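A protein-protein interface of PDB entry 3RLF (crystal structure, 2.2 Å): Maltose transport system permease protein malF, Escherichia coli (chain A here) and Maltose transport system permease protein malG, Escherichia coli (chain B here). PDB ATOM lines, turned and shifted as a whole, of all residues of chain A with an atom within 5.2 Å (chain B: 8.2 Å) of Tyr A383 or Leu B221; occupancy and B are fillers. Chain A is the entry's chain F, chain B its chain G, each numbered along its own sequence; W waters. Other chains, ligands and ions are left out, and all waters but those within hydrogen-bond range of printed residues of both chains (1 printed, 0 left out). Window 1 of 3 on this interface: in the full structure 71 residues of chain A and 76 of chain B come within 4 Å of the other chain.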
ATOM      1  N   TYR A 325      11.651  -1.980  -5.067  1.00  0.00           N
ATOM      2  CA  TYR A 325      10.736  -1.322  -5.988  1.00  0.00           C
ATOM      3  C   TYR A 325      11.132  -1.614  -7.437  1.00  0.00           C
ATOM      4  O   TYR A 325      10.373  -1.323  -8.367  1.00  0.00           O
ATOM      5  CB  TYR A 325      10.757   0.182  -5.708  1.00  0.00           C
ATOM      6  CG  TYR A 325       9.542   0.975  -6.149  1.00  0.00           C
ATOM      7  CD1 TYR A 325       8.315   0.359  -6.397  1.00  0.00           C
ATOM      8  CD2 TYR A 325       9.618   2.358  -6.276  1.00  0.00           C
ATOM      9  CE1 TYR A 325       7.203   1.106  -6.788  1.00  0.00           C
ATOM     10  CE2 TYR A 325       8.517   3.111  -6.656  1.00  0.00           C
ATOM     11  CZ  TYR A 325       7.316   2.483  -6.909  1.00  0.00           C
ATOM     12  OH  TYR A 325       6.237   3.241  -7.290  1.00  0.00           O
ATOM     13  N   LEU A 379       7.366  -2.793   0.586  1.00  0.00           N
ATOM     14  CA  LEU A 379       6.941  -2.447  -0.768  1.00  0.00           C
ATOM     15  C   LEU A 379       6.874  -0.936  -0.995  1.00  0.00           C
ATOM     16  O   LEU A 379       7.195  -0.446  -2.086  1.00  0.00           O
ATOM     17  CB  LEU A 379       5.562  -3.053  -1.063  1.00  0.00           C
ATOM     18  CG  LEU A 379       5.390  -4.564  -1.244  1.00  0.00           C
ATOM     19  CD1 LEU A 379       3.922  -4.937  -1.117  1.00  0.00           C
ATOM     20  CD2 LEU A 379       5.950  -5.018  -2.586  1.00  0.00           C
ATOM     21  N   GLY A 380       6.455  -0.210   0.040  1.00  0.00           N
ATOM     22  CA  GLY A 380       6.101   1.200  -0.087  1.00  0.00           C
ATOM     23  C   GLY A 380       7.165   2.240   0.203  1.00  0.00           C
ATOM     24  O   GLY A 380       7.138   3.328  -0.385  1.00  0.00           O
ATOM     25  N   TYR A 381       8.102   1.921   1.098  1.00  0.00           N
ATOM     26  CA  TYR A 381       9.124   2.893   1.522  1.00  0.00           C
ATOM     27  C   TYR A 381       9.987   3.478   0.381  1.00  0.00           C
ATOM     28  O   TYR A 381      10.315   4.663   0.427  1.00  0.00           O
ATOM     29  CB  TYR A 381       9.997   2.365   2.692  1.00  0.00           C
ATOM     30  CG  TYR A 381      11.197   1.523   2.286  1.00  0.00           C
ATOM     31  CD1 TYR A 381      12.332   2.115   1.721  1.00  0.00           C
ATOM     32  CD2 TYR A 381      11.204   0.142   2.476  1.00  0.00           C
ATOM     33  CE1 TYR A 381      13.424   1.355   1.332  1.00  0.00           C
ATOM     34  CE2 TYR A 381      12.302  -0.631   2.097  1.00  0.00           C
ATOM     35  CZ  TYR A 381      13.407  -0.013   1.524  1.00  0.00           C
ATOM     36  OH  TYR A 381      14.500  -0.755   1.142  1.00  0.00           O
ATOM     37  N   PRO A 382      10.356   2.665  -0.635  1.00  0.00           N
ATOM     38  CA  PRO A 382      11.232   3.220  -1.690  1.00  0.00           C
ATOM     39  C   PRO A 382      10.580   4.331  -2.516  1.00  0.00           C
ATOM     40  O   PRO A 382      11.263   5.280  -2.915  1.00  0.00           O
ATOM     41  CB  PRO A 382      11.535   2.002  -2.573  1.00  0.00           C
ATOM     42  CG  PRO A 382      11.308   0.819  -1.684  1.00  0.00           C
ATOM     43  CD  PRO A 382      10.132   1.220  -0.837  1.00  0.00           C
ATOM     44  N   TYR A 383       9.275   4.209  -2.761  1.00  0.00           N
ATOM     45  CA  TYR A 383       8.494   5.254  -3.428  1.00  0.00           C
ATOM     46  C   TYR A 383       8.656   6.594  -2.711  1.00  0.00           C
ATOM     47  O   TYR A 383       8.929   7.621  -3.343  1.00  0.00           O
ATOM     48  CB  TYR A 383       7.011   4.862  -3.453  1.00  0.00           C
ATOM     49  CG  TYR A 383       6.077   5.955  -3.918  1.00  0.00           C
ATOM     50  CD1 TYR A 383       5.976   6.282  -5.271  1.00  0.00           C
ATOM     51  CD2 TYR A 383       5.283   6.650  -3.011  1.00  0.00           C
ATOM     52  CE1 TYR A 383       5.117   7.279  -5.707  1.00  0.00           C
ATOM     53  CE2 TYR A 383       4.418   7.652  -3.438  1.00  0.00           C
ATOM     54  CZ  TYR A 383       4.341   7.959  -4.786  1.00  0.00           C
ATOM     55  OH  TYR A 383       3.489   8.943  -5.220  1.00  0.00           O
ATOM     56  N   MET A 384       8.482   6.562  -1.391  1.00  0.00           N
ATOM     57  CA  MET A 384       8.595   7.746  -0.550  1.00  0.00           C
ATOM     58  C   MET A 384      10.040   8.217  -0.466  1.00  0.00           C
ATOM     59  O   MET A 384      10.305   9.421  -0.426  1.00  0.00           O
ATOM     60  CB  MET A 384       8.046   7.464   0.854  1.00  0.00           C
ATOM     61  CG  MET A 384       6.532   7.288   0.914  1.00  0.00           C
ATOM     62  SD  MET A 384       5.678   8.784   0.381  1.00  0.00           S
ATOM     63  CE  MET A 384       3.962   8.286   0.558  1.00  0.00           C
ATOM     64  N   MET A 385      10.967   7.263  -0.442  1.00  0.00           N
ATOM     65  CA  MET A 385      12.394   7.578  -0.413  1.00  0.00           C
ATOM     66  C   MET A 385      12.810   8.350  -1.663  1.00  0.00           C
ATOM     67  O   MET A 385      13.505   9.361  -1.562  1.00  0.00           O
ATOM     68  CB  MET A 385      13.236   6.305  -0.261  1.00  0.00           C
ATOM     69  CG  MET A 385      14.724   6.570  -0.115  1.00  0.00           C
ATOM     70  SD  MET A 385      15.708   5.065  -0.156  1.00  0.00           S
ATOM     71  CE  MET A 385      17.340   5.753  -0.413  1.00  0.00           C
ATOM     72  N   ILE A 386      12.378   7.876  -2.831  1.00  0.00           N
ATOM     73  CA  ILE A 386      12.676   8.547  -4.103  1.00  0.00           C
ATOM     74  C   ILE A 386      12.101   9.969  -4.122  1.00  0.00           C
ATOM     75  O   ILE A 386      12.796  10.912  -4.494  1.00  0.00           O
ATOM     76  CB  ILE A 386      12.194   7.720  -5.328  1.00  0.00           C
ATOM     77  CG1 ILE A 386      13.039   6.447  -5.465  1.00  0.00           C
ATOM     78  CG2 ILE A 386      12.264   8.548  -6.616  1.00  0.00           C
ATOM     79  CD1 ILE A 386      12.328   5.276  -6.169  1.00  0.00           C
ATOM     80  N   LEU A 387      10.840  10.107  -3.708  1.00  0.00           N
ATOM     81  CA  LEU A 387      10.205  11.414  -3.545  1.00  0.00           C
ATOM     82  C   LEU A 387      11.043  12.336  -2.662  1.00  0.00           C
ATOM     83  O   LEU A 387      11.417  13.433  -3.084  1.00  0.00           O
ATOM     84  CB  LEU A 387       8.803  11.273  -2.943  1.00  0.00           C
ATOM     85  CG  LEU A 387       7.650  10.793  -3.823  1.00  0.00           C
ATOM     86  CD1 LEU A 387       6.416  10.639  -2.960  1.00  0.00           C
ATOM     87  CD2 LEU A 387       7.385  11.749  -4.973  1.00  0.00           C
ATOM     88  N   LEU A 429       0.828  14.092  -1.636  1.00  0.00           N
ATOM     89  CA  LEU A 429       1.364  12.762  -1.921  1.00  0.00           C
ATOM     90  C   LEU A 429       0.991  11.737  -0.846  1.00  0.00           C
ATOM     91  O   LEU A 429       0.751  10.573  -1.161  1.00  0.00           O
ATOM     92  CB  LEU A 429       2.882  12.824  -2.110  1.00  0.00           C
ATOM     93  CG  LEU A 429       3.374  13.574  -3.351  1.00  0.00           C
ATOM     94  CD1 LEU A 429       4.794  14.068  -3.158  1.00  0.00           C
ATOM     95  CD2 LEU A 429       3.258  12.714  -4.608  1.00  0.00           C
ATOM     96  N   ALA B  92       8.629   2.209 -21.630  1.00  0.00           N
ATOM     97  CA  ALA B  92       8.855   2.920 -20.365  1.00  0.00           C
ATOM     98  C   ALA B  92       9.608   4.241 -20.538  1.00  0.00           C
ATOM     99  O   ALA B  92       9.311   5.220 -19.852  1.00  0.00           O
ATOM    100  CB  ALA B  92       9.568   2.028 -19.355  1.00  0.00           C
ATOM    101  N   ALA B  96       7.850   7.892 -20.019  1.00  0.00           N
ATOM    102  CA  ALA B  96       8.380   8.696 -18.918  1.00  0.00           C
ATOM    103  C   ALA B  96       8.735  10.109 -19.387  1.00  0.00           C
ATOM    104  O   ALA B  96       8.455  11.084 -18.689  1.00  0.00           O
ATOM    105  CB  ALA B  96       9.586   8.015 -18.261  1.00  0.00           C
ATOM    106  N   ILE B  99       5.404  11.921 -19.884  1.00  0.00           N
ATOM    107  CA  ILE B  99       4.854  12.280 -18.576  1.00  0.00           C
ATOM    108  C   ILE B  99       5.580  13.490 -17.952  1.00  0.00           C
ATOM    109  O   ILE B  99       4.929  14.380 -17.421  1.00  0.00           O
ATOM    110  CB  ILE B  99       4.780  11.056 -17.623  1.00  0.00           C
ATOM    111  CG1 ILE B  99       3.655  10.113 -18.079  1.00  0.00           C
ATOM    112  CG2 ILE B  99       4.526  11.491 -16.181  1.00  0.00           C
ATOM    113  CD1 ILE B  99       3.806   8.665 -17.602  1.00  0.00           C
ATOM    114  N   VAL B 100       6.909  13.529 -18.036  1.00  0.00           N
ATOM    115  CA  VAL B 100       7.676  14.697 -17.582  1.00  0.00           C
ATOM    116  C   VAL B 100       7.341  15.954 -18.409  1.00  0.00           C
ATOM    117  O   VAL B 100       7.216  17.051 -17.856  1.00  0.00           O
ATOM    118  CB  VAL B 100       9.211  14.433 -17.579  1.00  0.00           C
ATOM    119  CG1 VAL B 100       9.989  15.700 -17.212  1.00  0.00           C
ATOM    120  CG2 VAL B 100       9.565  13.301 -16.613  1.00  0.00           C
ATOM    121  N   GLN B 129      -8.213  11.104 -10.210  1.00  0.00           N
ATOM    122  CA  GLN B 129      -7.189  10.067 -10.358  1.00  0.00           C
ATOM    123  C   GLN B 129      -7.301   9.024  -9.238  1.00  0.00           C
ATOM    124  O   GLN B 129      -6.795   7.906  -9.363  1.00  0.00           O
ATOM    125  CB  GLN B 129      -5.782  10.684 -10.424  1.00  0.00           C
ATOM    126  CG  GLN B 129      -4.692   9.709 -10.881  1.00  0.00           C
ATOM    127  CD  GLN B 129      -3.474  10.394 -11.477  1.00  0.00           C
ATOM    128  OE1 GLN B 129      -3.554  11.036 -12.530  1.00  0.00           O
ATOM    129  NE2 GLN B 129      -2.330  10.237 -10.819  1.00  0.00           N
ATOM    130  N   LEU B 172      -0.759  13.574 -10.058  1.00  0.00           N
ATOM    131  CA  LEU B 172       0.143  13.576  -8.903  1.00  0.00           C
ATOM    132  C   LEU B 172       1.495  14.214  -9.207  1.00  0.00           C
ATOM    133  O   LEU B 172       2.061  14.920  -8.366  1.00  0.00           O
ATOM    134  CB  LEU B 172       0.349  12.158  -8.372  1.00  0.00           C
ATOM    135  CG  LEU B 172      -0.565  11.721  -7.230  1.00  0.00           C
ATOM    136  CD1 LEU B 172      -0.303  10.259  -6.910  1.00  0.00           C
ATOM    137  CD2 LEU B 172      -0.343  12.596  -5.998  1.00  0.00           C
ATOM    138  N   HIS B 173       2.009  13.956 -10.406  1.00  0.00           N
ATOM    139  CA  HIS B 173       3.276  14.537 -10.833  1.00  0.00           C
ATOM    140  C   HIS B 173       3.168  16.050 -10.992  1.00  0.00           C
ATOM    141  O   HIS B 173       4.133  16.769 -10.724  1.00  0.00           O
ATOM    142  CB  HIS B 173       3.771  13.881 -12.123  1.00  0.00           C
ATOM    143  CG  HIS B 173       4.034  12.416 -11.985  1.00  0.00           C
ATOM    144  ND1 HIS B 173       4.720  11.880 -10.915  1.00  0.00           N
ATOM    145  CD2 HIS B 173       3.698  11.371 -12.778  1.00  0.00           C
ATOM    146  CE1 HIS B 173       4.800  10.569 -11.059  1.00  0.00           C
ATOM    147  NE2 HIS B 173       4.189  10.236 -12.181  1.00  0.00           N
ATOM    148  N   THR B 176       3.431  17.463  -7.496  1.00  0.00           N
ATOM    149  CA  THR B 176       4.805  17.252  -7.043  1.00  0.00           C
ATOM    150  C   THR B 176       5.755  18.309  -7.607  1.00  0.00           C
ATOM    151  O   THR B 176       6.557  18.886  -6.874  1.00  0.00           O
ATOM    152  CB  THR B 176       5.306  15.839  -7.438  1.00  0.00           C
ATOM    153  OG1 THR B 176       4.365  14.853  -6.995  1.00  0.00           O
ATOM    154  CG2 THR B 176       6.674  15.543  -6.828  1.00  0.00           C
ATOM    155  N   ILE B 214      13.572  17.304  -9.215  1.00  0.00           N
ATOM    156  CA  ILE B 214      12.204  16.777  -9.170  1.00  0.00           C
ATOM    157  C   ILE B 214      11.796  16.167 -10.513  1.00  0.00           C
ATOM    158  O   ILE B 214      10.937  15.292 -10.573  1.00  0.00           O
ATOM    159  CB  ILE B 214      11.164  17.831  -8.662  1.00  0.00           C
ATOM    160  CG1 ILE B 214       9.978  17.143  -7.980  1.00  0.00           C
ATOM    161  CG2 ILE B 214      10.698  18.762  -9.791  1.00  0.00           C
ATOM    162  CD1 ILE B 214      10.345  16.314  -6.724  1.00  0.00           C
ATOM    163  N   LEU B 215      12.430  16.631 -11.583  1.00  0.00           N
ATOM    164  CA  LEU B 215      12.225  16.064 -12.910  1.00  0.00           C
ATOM    165  C   LEU B 215      12.771  14.638 -12.958  1.00  0.00           C
ATOM    166  O   LEU B 215      12.162  13.754 -13.568  1.00  0.00           O
ATOM    167  CB  LEU B 215      12.904  16.935 -13.970  1.00  0.00           C
ATOM    168  CG  LEU B 215      12.491  18.406 -14.058  1.00  0.00           C
ATOM    169  CD1 LEU B 215      12.919  18.993 -15.403  1.00  0.00           C
ATOM    170  CD2 LEU B 215      10.990  18.579 -13.862  1.00  0.00           C
ATOM    171  N   ALA B 216      13.916  14.432 -12.309  1.00  0.00           N
ATOM    172  CA  ALA B 216      14.524  13.116 -12.155  1.00  0.00           C
ATOM    173  C   ALA B 216      13.585  12.169 -11.408  1.00  0.00           C
ATOM    174  O   ALA B 216      13.349  11.047 -11.854  1.00  0.00           O
ATOM    175  CB  ALA B 216      15.865  13.232 -11.424  1.00  0.00           C
ATOM    176  N   VAL B 217      13.046  12.633 -10.280  1.00  0.00           N
ATOM    177  CA  VAL B 217      12.082  11.859  -9.493  1.00  0.00           C
ATOM    178  C   VAL B 217      10.876  11.429 -10.344  1.00  0.00           C
ATOM    179  O   VAL B 217      10.488  10.264 -10.335  1.00  0.00           O
ATOM    180  CB  VAL B 217      11.605  12.645  -8.247  1.00  0.00           C
ATOM    181  CG1 VAL B 217      10.427  11.943  -7.564  1.00  0.00           C
ATOM    182  CG2 VAL B 217      12.751  12.817  -7.266  1.00  0.00           C
ATOM    183  N   VAL B 218      10.306  12.374 -11.084  1.00  0.00           N
ATOM    184  CA  VAL B 218       9.144  12.096 -11.915  1.00  0.00           C
ATOM    185  C   VAL B 218       9.505  11.099 -13.022  1.00  0.00           C
ATOM    186  O   VAL B 218       8.764  10.149 -13.257  1.00  0.00           O
ATOM    187  CB  VAL B 218       8.487  13.406 -12.453  1.00  0.00           C
ATOM    188  CG1 VAL B 218       7.424  13.113 -13.512  1.00  0.00           C
ATOM    189  CG2 VAL B 218       7.870  14.186 -11.303  1.00  0.00           C
ATOM    190  N   PHE B 219      10.659  11.282 -13.661  1.00  0.00           N
ATOM    191  CA  PHE B 219      11.139  10.288 -14.627  1.00  0.00           C
ATOM    192  C   PHE B 219      11.275   8.894 -13.999  1.00  0.00           C
ATOM    193  O   PHE B 219      10.721   7.922 -14.525  1.00  0.00           O
ATOM    194  CB  PHE B 219      12.458  10.710 -15.278  1.00  0.00           C
ATOM    195  CG  PHE B 219      12.820   9.883 -16.482  1.00  0.00           C
ATOM    196  CD1 PHE B 219      12.438  10.290 -17.758  1.00  0.00           C
ATOM    197  CD2 PHE B 219      13.517   8.684 -16.342  1.00  0.00           C
ATOM    198  CE1 PHE B 219      12.757   9.524 -18.879  1.00  0.00           C
ATOM    199  CE2 PHE B 219      13.843   7.908 -17.460  1.00  0.00           C
ATOM    200  CZ  PHE B 219      13.464   8.331 -18.729  1.00  0.00           C
ATOM    201  N   ILE B 220      12.001   8.804 -12.879  1.00  0.00           N
ATOM    202  CA  ILE B 220      12.229   7.523 -12.192  1.00  0.00           C
ATOM    203  C   ILE B 220      10.919   6.809 -11.863  1.00  0.00           C
ATOM    204  O   ILE B 220      10.780   5.617 -12.129  1.00  0.00           O
ATOM    205  CB  ILE B 220      13.059   7.684 -10.886  1.00  0.00           C
ATOM    206  CG1 ILE B 220      14.490   8.135 -11.189  1.00  0.00           C
ATOM    207  CG2 ILE B 220      13.114   6.371 -10.104  1.00  0.00           C
ATOM    208  CD1 ILE B 220      15.190   8.769  -9.977  1.00  0.00           C
ATOM    209  N   LEU B 221       9.964   7.543 -11.296  1.00  0.00           N
ATOM    210  CA  LEU B 221       8.707   6.941 -10.838  1.00  0.00           C
ATOM    211  C   LEU B 221       7.815   6.480 -11.986  1.00  0.00           C
ATOM    212  O   LEU B 221       7.142   5.455 -11.866  1.00  0.00           O
ATOM    213  CB  LEU B 221       7.937   7.896  -9.923  1.00  0.00           C
ATOM    214  CG  LEU B 221       8.514   8.236  -8.546  1.00  0.00           C
ATOM    215  CD1 LEU B 221       7.658   9.313  -7.894  1.00  0.00           C
ATOM    216  CD2 LEU B 221       8.626   7.013  -7.639  1.00  0.00           C
ATOM    217  N   SER B 222       7.811   7.249 -13.079  1.00  0.00           N
ATOM    218  CA  SER B 222       7.047   6.920 -14.287  1.00  0.00           C
ATOM    219  C   SER B 222       7.687   5.762 -15.038  1.00  0.00           C
ATOM    220  O   SER B 222       6.989   4.958 -15.654  1.00  0.00           O
ATOM    221  CB  SER B 222       6.978   8.115 -15.237  1.00  0.00           C
ATOM    222  OG  SER B 222       6.605   9.291 -14.560  1.00  0.00           O
ATOM    223  N   PHE B 223       9.016   5.708 -15.017  1.00  0.00           N
ATOM    224  CA  PHE B 223       9.744   4.637 -15.691  1.00  0.00           C
ATOM    225  C   PHE B 223       9.398   3.313 -15.013  1.00  0.00           C
ATOM    226  O   PHE B 223       9.039   2.346 -15.681  1.00  0.00           O
ATOM    227  CB  PHE B 223      11.256   4.904 -15.671  1.00  0.00           C
ATOM    228  CG  PHE B 223      12.050   3.995 -16.567  1.00  0.00           C
ATOM    229  CD1 PHE B 223      12.189   4.279 -17.924  1.00  0.00           C
ATOM    230  CD2 PHE B 223      12.672   2.855 -16.053  1.00  0.00           C
ATOM    231  CE1 PHE B 223      12.924   3.445 -18.756  1.00  0.00           C
ATOM    232  CE2 PHE B 223      13.412   2.011 -16.883  1.00  0.00           C
ATOM    233  CZ  PHE B 223      13.538   2.312 -18.240  1.00  0.00           C
ATOM    234  N   ILE B 224       9.470   3.308 -13.683  1.00  0.00           N
ATOM    235  CA  ILE B 224       9.186   2.134 -12.857  1.00  0.00           C
ATOM    236  C   ILE B 224       7.754   1.642 -13.049  1.00  0.00           C
ATOM    237  O   ILE B 224       7.539   0.463 -13.317  1.00  0.00           O
ATOM    238  CB  ILE B 224       9.472   2.417 -11.352  1.00  0.00           C
ATOM    239  CG1 ILE B 224      10.975   2.612 -11.128  1.00  0.00           C
ATOM    240  CG2 ILE B 224       8.931   1.293 -10.460  1.00  0.00           C
ATOM    241  CD1 ILE B 224      11.364   3.096  -9.733  1.00  0.00           C
ATOM    242  N   ALA B 225       6.784   2.547 -12.920  1.00  0.00           N
ATOM    243  CA  ALA B 225       5.375   2.199 -13.114  1.00  0.00           C
ATOM    244  C   ALA B 225       5.138   1.547 -14.479  1.00  0.00           C
ATOM    245  O   ALA B 225       4.345   0.615 -14.590  1.00  0.00           O
ATOM    246  CB  ALA B 225       4.480   3.425 -12.938  1.00  0.00           C
ATOM    247  N   ALA B 226       5.843   2.028 -15.501  1.00  0.00           N
ATOM    248  CA  ALA B 226       5.672   1.533 -16.868  1.00  0.00           C
ATOM    249  C   ALA B 226       6.374   0.203 -17.128  1.00  0.00           C
ATOM    250  O   ALA B 226       5.843  -0.645 -17.852  1.00  0.00           O
ATOM    251  CB  ALA B 226       6.115   2.581 -17.871  1.00  0.00           C
ATOM    252  N   ILE B 227       7.557   0.021 -16.543  1.00  0.00           N
ATOM    253  CA  ILE B 227       8.285  -1.249 -16.626  1.00  0.00           C
ATOM    254  C   ILE B 227       7.502  -2.409 -15.997  1.00  0.00           C
ATOM    255  O   ILE B 227       7.563  -3.540 -16.474  1.00  0.00           O
ATOM    256  CB  ILE B 227       9.688  -1.143 -15.963  1.00  0.00           C
ATOM    257  CG1 ILE B 227      10.678  -0.422 -16.890  1.00  0.00           C
ATOM    258  CG2 ILE B 227      10.227  -2.530 -15.538  1.00  0.00           C
ATOM    259  CD1 ILE B 227      11.083  -1.186 -18.149  1.00  0.00           C
ATOM    260  N   THR B 228       6.772  -2.123 -14.927  1.00  0.00           N
ATOM    261  CA  THR B 228       6.091  -3.170 -14.169  1.00  0.00           C
ATOM    262  C   THR B 228       4.608  -3.334 -14.536  1.00  0.00           C
ATOM    263  O   THR B 228       3.947  -4.236 -14.035  1.00  0.00           O
ATOM    264  CB  THR B 228       6.230  -2.931 -12.653  1.00  0.00           C
ATOM    265  OG1 THR B 228       5.638  -1.671 -12.309  1.00  0.00           O
ATOM    266  CG2 THR B 228       7.708  -2.929 -12.241  1.00  0.00           C
ATOM    267  N   ILE B 274      15.635  -0.392 -14.552  1.00  0.00           N
ATOM    268  CA  ILE B 274      15.264   0.449 -13.406  1.00  0.00           C
ATOM    269  C   ILE B 274      16.521   0.926 -12.687  1.00  0.00           C
ATOM    270  O   ILE B 274      16.674   2.109 -12.395  1.00  0.00           O
ATOM    271  CB  ILE B 274      14.389  -0.335 -12.381  1.00  0.00           C
ATOM    272  CG1 ILE B 274      13.135  -0.897 -13.047  1.00  0.00           C
ATOM    273  CG2 ILE B 274      14.005   0.542 -11.195  1.00  0.00           C
ATOM    274  CD1 ILE B 274      12.239   0.154 -13.582  1.00  0.00           C
ATOM    275  N   VAL B 277      18.509   3.373 -14.862  1.00  0.00           N
ATOM    276  CA  VAL B 277      17.835   4.674 -14.877  1.00  0.00           C
ATOM    277  C   VAL B 277      18.001   5.397 -13.534  1.00  0.00           C
ATOM    278  O   VAL B 277      18.264   6.597 -13.505  1.00  0.00           O
ATOM    279  CB  VAL B 277      16.350   4.564 -15.335  1.00  0.00           C
ATOM    280  CG1 VAL B 277      15.549   5.810 -14.961  1.00  0.00           C
ATOM    281  CG2 VAL B 277      16.287   4.337 -16.835  1.00  0.00           C
ATOM    282  N   PHE B 278      17.895   4.663 -12.430  1.00  0.00           N
ATOM    283  CA  PHE B 278      18.119   5.255 -11.114  1.00  0.00           C
ATOM    284  C   PHE B 278      19.533   5.830 -10.973  1.00  0.00           C
ATOM    285  O   PHE B 278      19.711   6.904 -10.394  1.00  0.00           O
ATOM    286  CB  PHE B 278      17.827   4.255  -9.995  1.00  0.00           C
ATOM    287  CG  PHE B 278      18.045   4.808  -8.614  1.00  0.00           C
ATOM    288  CD1 PHE B 278      17.173   5.759  -8.084  1.00  0.00           C
ATOM    289  CD2 PHE B 278      19.120   4.375  -7.839  1.00  0.00           C
ATOM    290  CE1 PHE B 278      17.369   6.273  -6.806  1.00  0.00           C
ATOM    291  CE2 PHE B 278      19.329   4.885  -6.559  1.00  0.00           C
ATOM    292  CZ  PHE B 278      18.452   5.833  -6.038  1.00  0.00           C
HETATM  293  O   HOH W   1       5.988   4.600  -9.593  1.00  0.00           O
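The side-chain hydroxyl (OG1) of Thr B176 lies within hydrogen-bond range of the backbone carbonyl oxygen (O) of Leu B172 (2.7 Å). O of Ile B224 sits at hydrogen-bond distance from OG1 of Thr B228 (3.0 Å).
Among the printed residues, pairs that only touch across the chains: Tyr A325 with Ile B224 (3.6 Å), Tyr A383 with Leu B221 (3.6 Å), Ile A386 with Val B217 (3.4 Å), Leu A387 with Leu B221 (3.8 Å), Leu A429 with Leu B172 (3.9 Å) and Leu A429 with Thr B176 (3.4 Å).
Of the printed residues of chain B, Tyr A383 touches Leu B221 (3.6 Å). Of chain A, only Tyr A383 (3.6 Å) and Leu A387 (3.8 Å) come within 4 Å of Leu B221. No residue of chain B comes within 4 Å of Pro A382. Printed residues of chain A within 4 Å of Leu B172: Leu A429. Of the printed residues of chain A, Val B217 touches Ile A386. Of the printed residues of chain B, Leu A429 touches Leu B172 (3.9 Å) and Thr B176 (3.4 Å). Printed residues of chain B within 4 Å of Tyr A325: Ile B224. Of the printed residues of chain A, Ile B224 touches Tyr A325 (3.6 Å). Ile B99 touches none of the printed residues of chain A. Phe B278 touches none of the printed residues of chain A. The nearest printed residue of chain B that does not touch Tyr A325 is Leu B221 (4.03 Å).
Hydrophobic or aromatic side chains of chain B within 4 Å of the printed part of chain A: Leu B172, Val B217, Leu B221 and Ile B224. Of the 11 printed residues of chain A, 5 touch a printed residue of chain B. Among the printed residues, 6 pairs touch across the chains. Among the printed residues, no Asp or Glu carboxylate lies within 4 Å of a Lys or Arg side-chain nitrogen of the other chain.
Water W1 bridges the side-chain hydroxyl of Tyr A325 (2.7 Å) and the backbone carbonyl oxygen of Leu B221 (2.7 Å).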
